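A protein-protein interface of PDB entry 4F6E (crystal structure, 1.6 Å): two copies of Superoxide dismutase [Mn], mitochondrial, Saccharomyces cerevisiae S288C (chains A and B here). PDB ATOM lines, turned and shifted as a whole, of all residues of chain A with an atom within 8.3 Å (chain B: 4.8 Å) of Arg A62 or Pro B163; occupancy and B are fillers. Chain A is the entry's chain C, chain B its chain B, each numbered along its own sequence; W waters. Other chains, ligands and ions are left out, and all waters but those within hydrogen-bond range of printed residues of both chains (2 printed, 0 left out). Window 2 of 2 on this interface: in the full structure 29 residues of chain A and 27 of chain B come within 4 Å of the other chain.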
ATOM      1  N   LEU A  48      -7.204   6.867  19.471  1.00  0.00           N
ATOM      2  CA  LEU A  48      -6.037   7.565  20.013  1.00  0.00           C
ATOM      3  C   LEU A  48      -6.278   9.058  20.166  1.00  0.00           C
ATOM      4  O   LEU A  48      -5.752   9.683  21.091  1.00  0.00           O
ATOM      5  CB  LEU A  48      -4.806   7.322  19.140  1.00  0.00           C
ATOM      6  CG  LEU A  48      -4.211   5.918  19.212  1.00  0.00           C
ATOM      7  CD1 LEU A  48      -2.976   5.884  18.376  1.00  0.00           C
ATOM      8  CD2 LEU A  48      -3.872   5.513  20.645  1.00  0.00           C
ATOM      9  N   LEU A  52      -5.832  10.960  23.532  1.00  0.00           N
ATOM     10  CA  LEU A  52      -4.952  12.124  23.624  1.00  0.00           C
ATOM     11  C   LEU A  52      -5.651  13.331  24.260  1.00  0.00           C
ATOM     12  O   LEU A  52      -5.031  14.102  24.993  1.00  0.00           O
ATOM     13  CB  LEU A  52      -4.412  12.491  22.236  1.00  0.00           C
ATOM     14  CG  LEU A  52      -3.292  13.532  22.206  1.00  0.00           C
ATOM     15  CD1 LEU A  52      -1.997  12.964  22.769  1.00  0.00           C
ATOM     16  CD2 LEU A  52      -3.087  14.064  20.801  1.00  0.00           C
ATOM     17  N   SER A  57      -0.261  13.241  26.629  1.00  0.00           N
ATOM     18  CA  SER A  57       1.120  12.916  26.953  1.00  0.00           C
ATOM     19  C   SER A  57       1.963  12.658  25.711  1.00  0.00           C
ATOM     20  O   SER A  57       1.431  12.340  24.650  1.00  0.00           O
ATOM     21  CB  SER A  57       1.152  11.671  27.833  1.00  0.00           C
ATOM     22  OG  SER A  57       0.668  10.551  27.115  1.00  0.00           O
ATOM     23  N   PRO A  58       3.291  12.800  25.834  1.00  0.00           N
ATOM     24  CA  PRO A  58       4.198  12.364  24.772  1.00  0.00           C
ATOM     25  C   PRO A  58       4.028  10.880  24.432  1.00  0.00           C
ATOM     26  O   PRO A  58       4.155  10.507  23.266  1.00  0.00           O
ATOM     27  CB  PRO A  58       5.582  12.622  25.374  1.00  0.00           C
ATOM     28  CG  PRO A  58       5.365  13.749  26.318  1.00  0.00           C
ATOM     29  CD  PRO A  58       3.993  13.557  26.889  1.00  0.00           C
ATOM     30  N   ALA A  59       3.752  10.043  25.432  1.00  0.00           N
ATOM     31  CA  ALA A  59       3.562   8.617  25.174  1.00  0.00           C
ATOM     32  C   ALA A  59       2.379   8.381  24.237  1.00  0.00           C
ATOM     33  O   ALA A  59       2.451   7.557  23.329  1.00  0.00           O
ATOM     34  CB  ALA A  59       3.363   7.850  26.481  1.00  0.00           C
ATOM     35  N   ASN A  60       1.295   9.112  24.466  1.00  0.00           N
ATOM     36  CA  ASN A  60       0.112   8.954  23.628  1.00  0.00           C
ATOM     37  C   ASN A  60       0.297   9.561  22.234  1.00  0.00           C
ATOM     38  O   ASN A  60      -0.211   9.035  21.244  1.00  0.00           O
ATOM     39  CB  ASN A  60      -1.128   9.515  24.329  1.00  0.00           C
ATOM     40  CG  ASN A  60      -1.606   8.616  25.465  1.00  0.00           C
ATOM     41  OD1 ASN A  60      -1.364   7.406  25.451  1.00  0.00           O
ATOM     42  ND2 ASN A  60      -2.283   9.202  26.449  1.00  0.00           N
ATOM     43  N   ALA A  61       1.043  10.653  22.147  1.00  0.00           N
ATOM     44  CA  ALA A  61       1.345  11.238  20.841  1.00  0.00           C
ATOM     45  C   ALA A  61       2.234  10.290  20.033  1.00  0.00           C
ATOM     46  O   ALA A  61       2.122  10.197  18.810  1.00  0.00           O
ATOM     47  CB  ALA A  61       2.008  12.589  21.008  1.00  0.00           C
ATOM     48  N   ARG A  62       3.114   9.582  20.736  1.00  0.00           N
ATOM     49  CA  ARG A  62       3.972   8.567  20.144  1.00  0.00           C
ATOM     50  C   ARG A  62       3.143   7.440  19.495  1.00  0.00           C
ATOM     51  O   ARG A  62       3.471   6.970  18.410  1.00  0.00           O
ATOM     52  CB  ARG A  62       4.913   8.024  21.229  1.00  0.00           C
ATOM     53  CG  ARG A  62       6.053   7.129  20.776  1.00  0.00           C
ATOM     54  CD  ARG A  62       6.994   6.856  21.973  1.00  0.00           C
ATOM     55  NE  ARG A  62       7.915   5.734  21.771  1.00  0.00           N
ATOM     56  CZ  ARG A  62       7.682   4.489  22.181  1.00  0.00           C
ATOM     57  NH1 ARG A  62       6.551   4.196  22.813  1.00  0.00           N
ATOM     58  NH2 ARG A  62       8.579   3.532  21.962  1.00  0.00           N
ATOM     59  N   MLY A  63       2.072   7.021  20.165  1.00  0.00           N
ATOM     60  CA  MLY A  63       1.190   5.994  19.616  1.00  0.00           C
ATOM     61  CB  MLY A  63       0.149   5.565  20.644  1.00  0.00           C
ATOM     62  CG  MLY A  63       0.720   4.939  21.909  1.00  0.00           C
ATOM     63  CD  MLY A  63      -0.402   4.362  22.759  1.00  0.00           C
ATOM     64  CE  MLY A  63       0.122   3.634  23.989  1.00  0.00           C
ATOM     65  NZ  MLY A  63      -0.953   2.819  24.622  1.00  0.00           N
ATOM     66  CH1 MLY A  63      -0.378   2.245  25.846  1.00  0.00           C
ATOM     67  CH2 MLY A  63      -2.026   3.739  25.028  1.00  0.00           C
ATOM     68  C   MLY A  63       0.487   6.507  18.361  1.00  0.00           C
ATOM     69  O   MLY A  63       0.308   5.768  17.386  1.00  0.00           O
ATOM     70  N   MET A  64       0.099   7.776  18.392  1.00  0.00           N
ATOM     71  CA  MET A  64      -0.508   8.411  17.229  1.00  0.00           C
ATOM     72  C   MET A  64       0.442   8.463  16.035  1.00  0.00           C
ATOM     73  O   MET A  64       0.050   8.176  14.903  1.00  0.00           O
ATOM     74  CB  MET A  64      -0.975   9.812  17.600  1.00  0.00           C
ATOM     75  CG  MET A  64      -2.460   9.952  17.632  1.00  0.00           C
ATOM     76  SD  MET A  64      -3.247  10.197  16.019  1.00  0.00           S
ATOM     77  CE  MET A  64      -4.654  11.078  16.692  1.00  0.00           C
ATOM     78  N   ILE A  65       1.701   8.814  16.287  1.00  0.00           N
ATOM     79  CA  ILE A  65       2.709   8.816  15.233  1.00  0.00           C
ATOM     80  C   ILE A  65       2.826   7.441  14.582  1.00  0.00           C
ATOM     81  O   ILE A  65       2.947   7.317  13.367  1.00  0.00           O
ATOM     82  CB  ILE A  65       4.088   9.235  15.803  1.00  0.00           C
ATOM     83  CG1 ILE A  65       4.044  10.696  16.245  1.00  0.00           C
ATOM     84  CG2 ILE A  65       5.195   9.002  14.794  1.00  0.00           C
ATOM     85  CD1 ILE A  65       5.253  11.101  17.074  1.00  0.00           C
ATOM     86  N   ALA A  66       2.773   6.399  15.403  1.00  0.00           N
ATOM     87  CA  ALA A  66       2.946   5.046  14.902  1.00  0.00           C
ATOM     88  C   ALA A  66       1.870   4.638  13.899  1.00  0.00           C
ATOM     89  O   ALA A  66       2.130   3.837  13.003  1.00  0.00           O
ATOM     90  CB  ALA A  66       2.990   4.057  16.069  1.00  0.00           C
ATOM     91  N   ILE A  67       0.665   5.185  14.052  1.00  0.00           N
ATOM     92  CA  ILE A  67      -0.475   4.793  13.202  1.00  0.00           C
ATOM     93  C   ILE A  67      -0.502   5.565  11.873  1.00  0.00           C
ATOM     94  O   ILE A  67      -1.135   5.139  10.894  1.00  0.00           O
ATOM     95  CB  ILE A  67      -1.797   4.941  13.982  1.00  0.00           C
ATOM     96  CG1 ILE A  67      -1.731   4.030  15.210  1.00  0.00           C
ATOM     97  CG2 ILE A  67      -3.021   4.607  13.131  1.00  0.00           C
ATOM     98  CD1 ILE A  67      -3.037   3.705  15.808  1.00  0.00           C
ATOM     99  N   GLN A  68       0.224   6.677  11.830  1.00  0.00           N
ATOM    100  CA  GLN A  68       0.259   7.532  10.645  1.00  0.00           C
ATOM    101  C   GLN A  68       0.710   6.783   9.404  1.00  0.00           C
ATOM    102  O   GLN A  68       0.176   7.020   8.318  1.00  0.00           O
ATOM    103  CB  GLN A  68       1.189   8.727  10.864  1.00  0.00           C
ATOM    104  CG  GLN A  68       0.709   9.663  11.924  1.00  0.00           C
ATOM    105  CD  GLN A  68      -0.776   9.925  11.795  1.00  0.00           C
ATOM    106  OE1 GLN A  68      -1.242  10.431  10.774  1.00  0.00           O
ATOM    107  NE2 GLN A  68      -1.532   9.569  12.827  1.00  0.00           N
ATOM    108  N   THR B  79       6.956  15.292  20.685  1.00  0.00           N
ATOM    109  CA  THR B  79       7.401  14.221  21.578  1.00  0.00           C
ATOM    110  C   THR B  79       8.914  14.194  21.748  1.00  0.00           C
ATOM    111  O   THR B  79       9.390  14.017  22.863  1.00  0.00           O
ATOM    112  CB  THR B  79       6.925  12.850  21.089  1.00  0.00           C
ATOM    113  OG1 THR B  79       7.486  12.580  19.811  1.00  0.00           O
ATOM    114  CG2 THR B  79       5.437  12.835  20.955  1.00  0.00           C
ATOM    115  N   LEU B  83      11.009  14.565  25.351  1.00  0.00           N
ATOM    116  CA  LEU B  83      12.041  13.633  25.805  1.00  0.00           C
ATOM    117  C   LEU B  83      13.351  14.355  26.105  1.00  0.00           C
ATOM    118  O   LEU B  83      13.978  14.115  27.136  1.00  0.00           O
ATOM    119  CB  LEU B  83      12.278  12.561  24.742  1.00  0.00           C
ATOM    120  CG  LEU B  83      11.131  11.584  24.499  1.00  0.00           C
ATOM    121  CD1 LEU B  83      11.469  10.729  23.288  1.00  0.00           C
ATOM    122  CD2 LEU B  83      10.905  10.710  25.728  1.00  0.00           C
ATOM    123  N   PHE B 135      19.006   8.369  19.332  1.00  0.00           N
ATOM    124  CA  PHE B 135      18.376   7.885  20.555  1.00  0.00           C
ATOM    125  C   PHE B 135      19.133   6.675  21.071  1.00  0.00           C
ATOM    126  O   PHE B 135      19.401   5.740  20.310  1.00  0.00           O
ATOM    127  CB  PHE B 135      16.926   7.445  20.313  1.00  0.00           C
ATOM    128  CG  PHE B 135      16.026   8.525  19.776  1.00  0.00           C
ATOM    129  CD1 PHE B 135      15.263   9.301  20.635  1.00  0.00           C
ATOM    130  CD2 PHE B 135      15.911   8.731  18.407  1.00  0.00           C
ATOM    131  CE1 PHE B 135      14.427  10.282  20.137  1.00  0.00           C
ATOM    132  CE2 PHE B 135      15.077   9.704  17.901  1.00  0.00           C
ATOM    133  CZ  PHE B 135      14.331  10.481  18.765  1.00  0.00           C
ATOM    134  N   ILE B 136      19.460   6.681  22.360  1.00  0.00           N
ATOM    135  CA  ILE B 136      19.859   5.454  23.024  1.00  0.00           C
ATOM    136  C   ILE B 136      18.556   4.784  23.435  1.00  0.00           C
ATOM    137  O   ILE B 136      17.715   5.401  24.095  1.00  0.00           O
ATOM    138  CB  ILE B 136      20.754   5.731  24.248  1.00  0.00           C
ATOM    139  CG1 ILE B 136      22.027   6.461  23.800  1.00  0.00           C
ATOM    140  CG2 ILE B 136      21.118   4.423  24.941  1.00  0.00           C
ATOM    141  CD1 ILE B 136      23.000   6.802  24.947  1.00  0.00           C
ATOM    142  N   VAL B 137      18.362   3.536  23.022  1.00  0.00           N
ATOM    143  CA  VAL B 137      17.067   2.886  23.211  1.00  0.00           C
ATOM    144  C   VAL B 137      17.184   1.564  23.945  1.00  0.00           C
ATOM    145  O   VAL B 137      18.260   0.958  23.974  1.00  0.00           O
ATOM    146  CB  VAL B 137      16.368   2.597  21.852  1.00  0.00           C
ATOM    147  CG1 VAL B 137      16.102   3.890  21.085  1.00  0.00           C
ATOM    148  CG2 VAL B 137      17.223   1.678  21.005  1.00  0.00           C
ATOM    149  N   VAL B 157      11.403   7.145  17.607  1.00  0.00           N
ATOM    150  CA  VAL B 157      11.350   5.715  17.867  1.00  0.00           C
ATOM    151  C   VAL B 157      10.015   5.359  18.500  1.00  0.00           C
ATOM    152  O   VAL B 157       9.552   6.032  19.419  1.00  0.00           O
ATOM    153  CB  VAL B 157      12.531   5.251  18.760  1.00  0.00           C
ATOM    154  CG1 VAL B 157      13.824   5.380  17.988  1.00  0.00           C
ATOM    155  CG2 VAL B 157      12.600   6.073  20.039  1.00  0.00           C
ATOM    156  N   THR B 158       9.384   4.313  17.986  1.00  0.00           N
ATOM    157  CA  THR B 158       8.063   3.926  18.455  1.00  0.00           C
ATOM    158  C   THR B 158       8.029   2.431  18.713  1.00  0.00           C
ATOM    159  O   THR B 158       9.028   1.729  18.517  1.00  0.00           O
ATOM    160  CB  THR B 158       6.976   4.259  17.413  1.00  0.00           C
ATOM    161  OG1 THR B 158       7.267   3.575  16.190  1.00  0.00           O
ATOM    162  CG2 THR B 158       6.914   5.764  17.150  1.00  0.00           C
ATOM    163  N   GLY B 159       6.863   1.950  19.133  1.00  0.00           N
ATOM    164  CA  GLY B 159       6.672   0.539  19.394  1.00  0.00           C
ATOM    165  C   GLY B 159       7.634   0.018  20.439  1.00  0.00           C
ATOM    166  O   GLY B 159       7.747   0.596  21.526  1.00  0.00           O
ATOM    167  N   LEU B 161      10.832   0.078  20.561  1.00  0.00           N
ATOM    168  CA  LEU B 161      12.056   0.833  20.809  1.00  0.00           C
ATOM    169  C   LEU B 161      11.768   1.950  21.799  1.00  0.00           C
ATOM    170  O   LEU B 161      11.204   2.983  21.422  1.00  0.00           O
ATOM    171  CB  LEU B 161      12.640   1.407  19.520  1.00  0.00           C
ATOM    172  CG  LEU B 161      13.165   0.404  18.492  1.00  0.00           C
ATOM    173  CD1 LEU B 161      13.818   1.135  17.327  1.00  0.00           C
ATOM    174  CD2 LEU B 161      14.152  -0.563  19.139  1.00  0.00           C
ATOM    175  N   VAL B 162      12.153   1.734  23.054  1.00  0.00           N
ATOM    176  CA  VAL B 162      11.907   2.704  24.124  1.00  0.00           C
ATOM    177  C   VAL B 162      13.052   3.710  24.213  1.00  0.00           C
ATOM    178  O   VAL B 162      14.206   3.333  24.421  1.00  0.00           O
ATOM    179  CB  VAL B 162      11.766   2.004  25.486  1.00  0.00           C
ATOM    180  CG1 VAL B 162      11.496   3.032  26.575  1.00  0.00           C
ATOM    181  CG2 VAL B 162      10.654   0.967  25.445  1.00  0.00           C
ATOM    182  N   PRO B 163      12.746   5.005  24.050  1.00  0.00           N
ATOM    183  CA  PRO B 163      13.839   5.979  24.113  1.00  0.00           C
ATOM    184  C   PRO B 163      14.318   6.189  25.544  1.00  0.00           C
ATOM    185  O   PRO B 163      13.517   6.418  26.455  1.00  0.00           O
ATOM    186  CB  PRO B 163      13.206   7.262  23.538  1.00  0.00           C
ATOM    187  CG  PRO B 163      11.740   7.097  23.774  1.00  0.00           C
ATOM    188  CD  PRO B 163      11.442   5.624  23.759  1.00  0.00           C
ATOM    189  N   LEU B 164      15.630   6.091  25.736  1.00  0.00           N
ATOM    190  CA  LEU B 164      16.230   6.330  27.046  1.00  0.00           C
ATOM    191  C   LEU B 164      16.921   7.683  27.073  1.00  0.00           C
ATOM    192  O   LEU B 164      16.796   8.429  28.051  1.00  0.00           O
ATOM    193  CB  LEU B 164      17.239   5.230  27.390  1.00  0.00           C
ATOM    194  CG  LEU B 164      16.719   3.818  27.143  1.00  0.00           C
ATOM    195  CD1 LEU B 164      17.806   2.817  27.453  1.00  0.00           C
ATOM    196  CD2 LEU B 164      15.494   3.556  27.998  1.00  0.00           C
ATOM    197  N   VAL B 165      17.677   7.991  26.019  1.00  0.00           N
ATOM    198  CA  VAL B 165      18.315   9.302  25.887  1.00  0.00           C
ATOM    199  C   VAL B 165      18.099   9.789  24.465  1.00  0.00           C
ATOM    200  O   VAL B 165      18.435   9.094  23.509  1.00  0.00           O
ATOM    201  CB  VAL B 165      19.837   9.267  26.193  1.00  0.00           C
ATOM    202  CG1 VAL B 165      20.473  10.644  25.944  1.00  0.00           C
ATOM    203  CG2 VAL B 165      20.100   8.826  27.633  1.00  0.00           C
ATOM    204  N   ARG B 201      13.586   5.480  32.675  1.00  0.00           N
ATOM    205  CA  ARG B 201      12.985   5.004  31.433  1.00  0.00           C
ATOM    206  C   ARG B 201      13.324   3.541  31.136  1.00  0.00           C
ATOM    207  O   ARG B 201      12.484   2.780  30.642  1.00  0.00           O
ATOM    208  CB  ARG B 201      13.430   5.892  30.265  1.00  0.00           C
ATOM    209  CG  ARG B 201      12.902   7.307  30.334  1.00  0.00           C
ATOM    210  CD  ARG B 201      13.614   8.195  29.326  1.00  0.00           C
ATOM    211  NE  ARG B 201      13.079   9.552  29.327  1.00  0.00           N
ATOM    212  CZ  ARG B 201      13.590  10.547  28.608  1.00  0.00           C
ATOM    213  NH1 ARG B 201      14.654  10.334  27.839  1.00  0.00           N
ATOM    214  NH2 ARG B 201      13.041  11.750  28.668  1.00  0.00           N
HETATM  215  O   HOH W   1       4.566   3.599  20.251  1.00  0.00           O
HETATM  216  O   HOH W   2       9.620   8.341  20.908  1.00  0.00           O
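Of the 14 printed residues of chain B, 6 touch a printed residue of chain A.
Printed residues of chain B that touch a printed residue of chain A: Thr B79, Val B157, Thr B158, Gly B159, Leu B161 and Pro B163.
Hydrophobic or aromatic side chains of chain B within 4 Å of the printed part of chain A: Pro B163.
Pro A58 touches Thr B79 (O to CG2, 3.5 Å).
Ala A61 touches Thr B79 (CB to CG2, 3.4 Å).
Thr B158 touches Arg A62.
Pro B163 touches Arg A62 (CD to NH2, 3.98 Å).
Thr B79 touches Ile A65.
NE of Arg A62 lies within hydrogen-bond range of O of Val B157, 2.9 Å away.
NH2 of Arg A62 sits at hydrogen-bond distance from O of Gly B159.
The backbone carbonyl oxygen of Leu B161 lies within hydrogen-bond range of the guanidinium group of Arg A62 (2.7 Å).
No position is printed for both chains.
Water W2 bridges O of Val B157 (2.7 Å) and NE of Arg A62 (3.2 Å).
Water W1 lies within hydrogen-bond range of N of Gly B159 (3.0 Å) and NH1 of Arg A62 (3.3 Å).
Of the printed residues of chain B, Pro A58 touches Thr B79.
Printed residues of chain B within 4 Å of Arg A62: Val B157, Thr B158, Gly B159, Leu B161 and Pro B163.
Of the printed residues of chain B, Ile A65 touches Thr B79.
Printed residues of chain A within 4 Å of Gly B159: Arg A62.
Pro B163 touches one residue of chain A.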
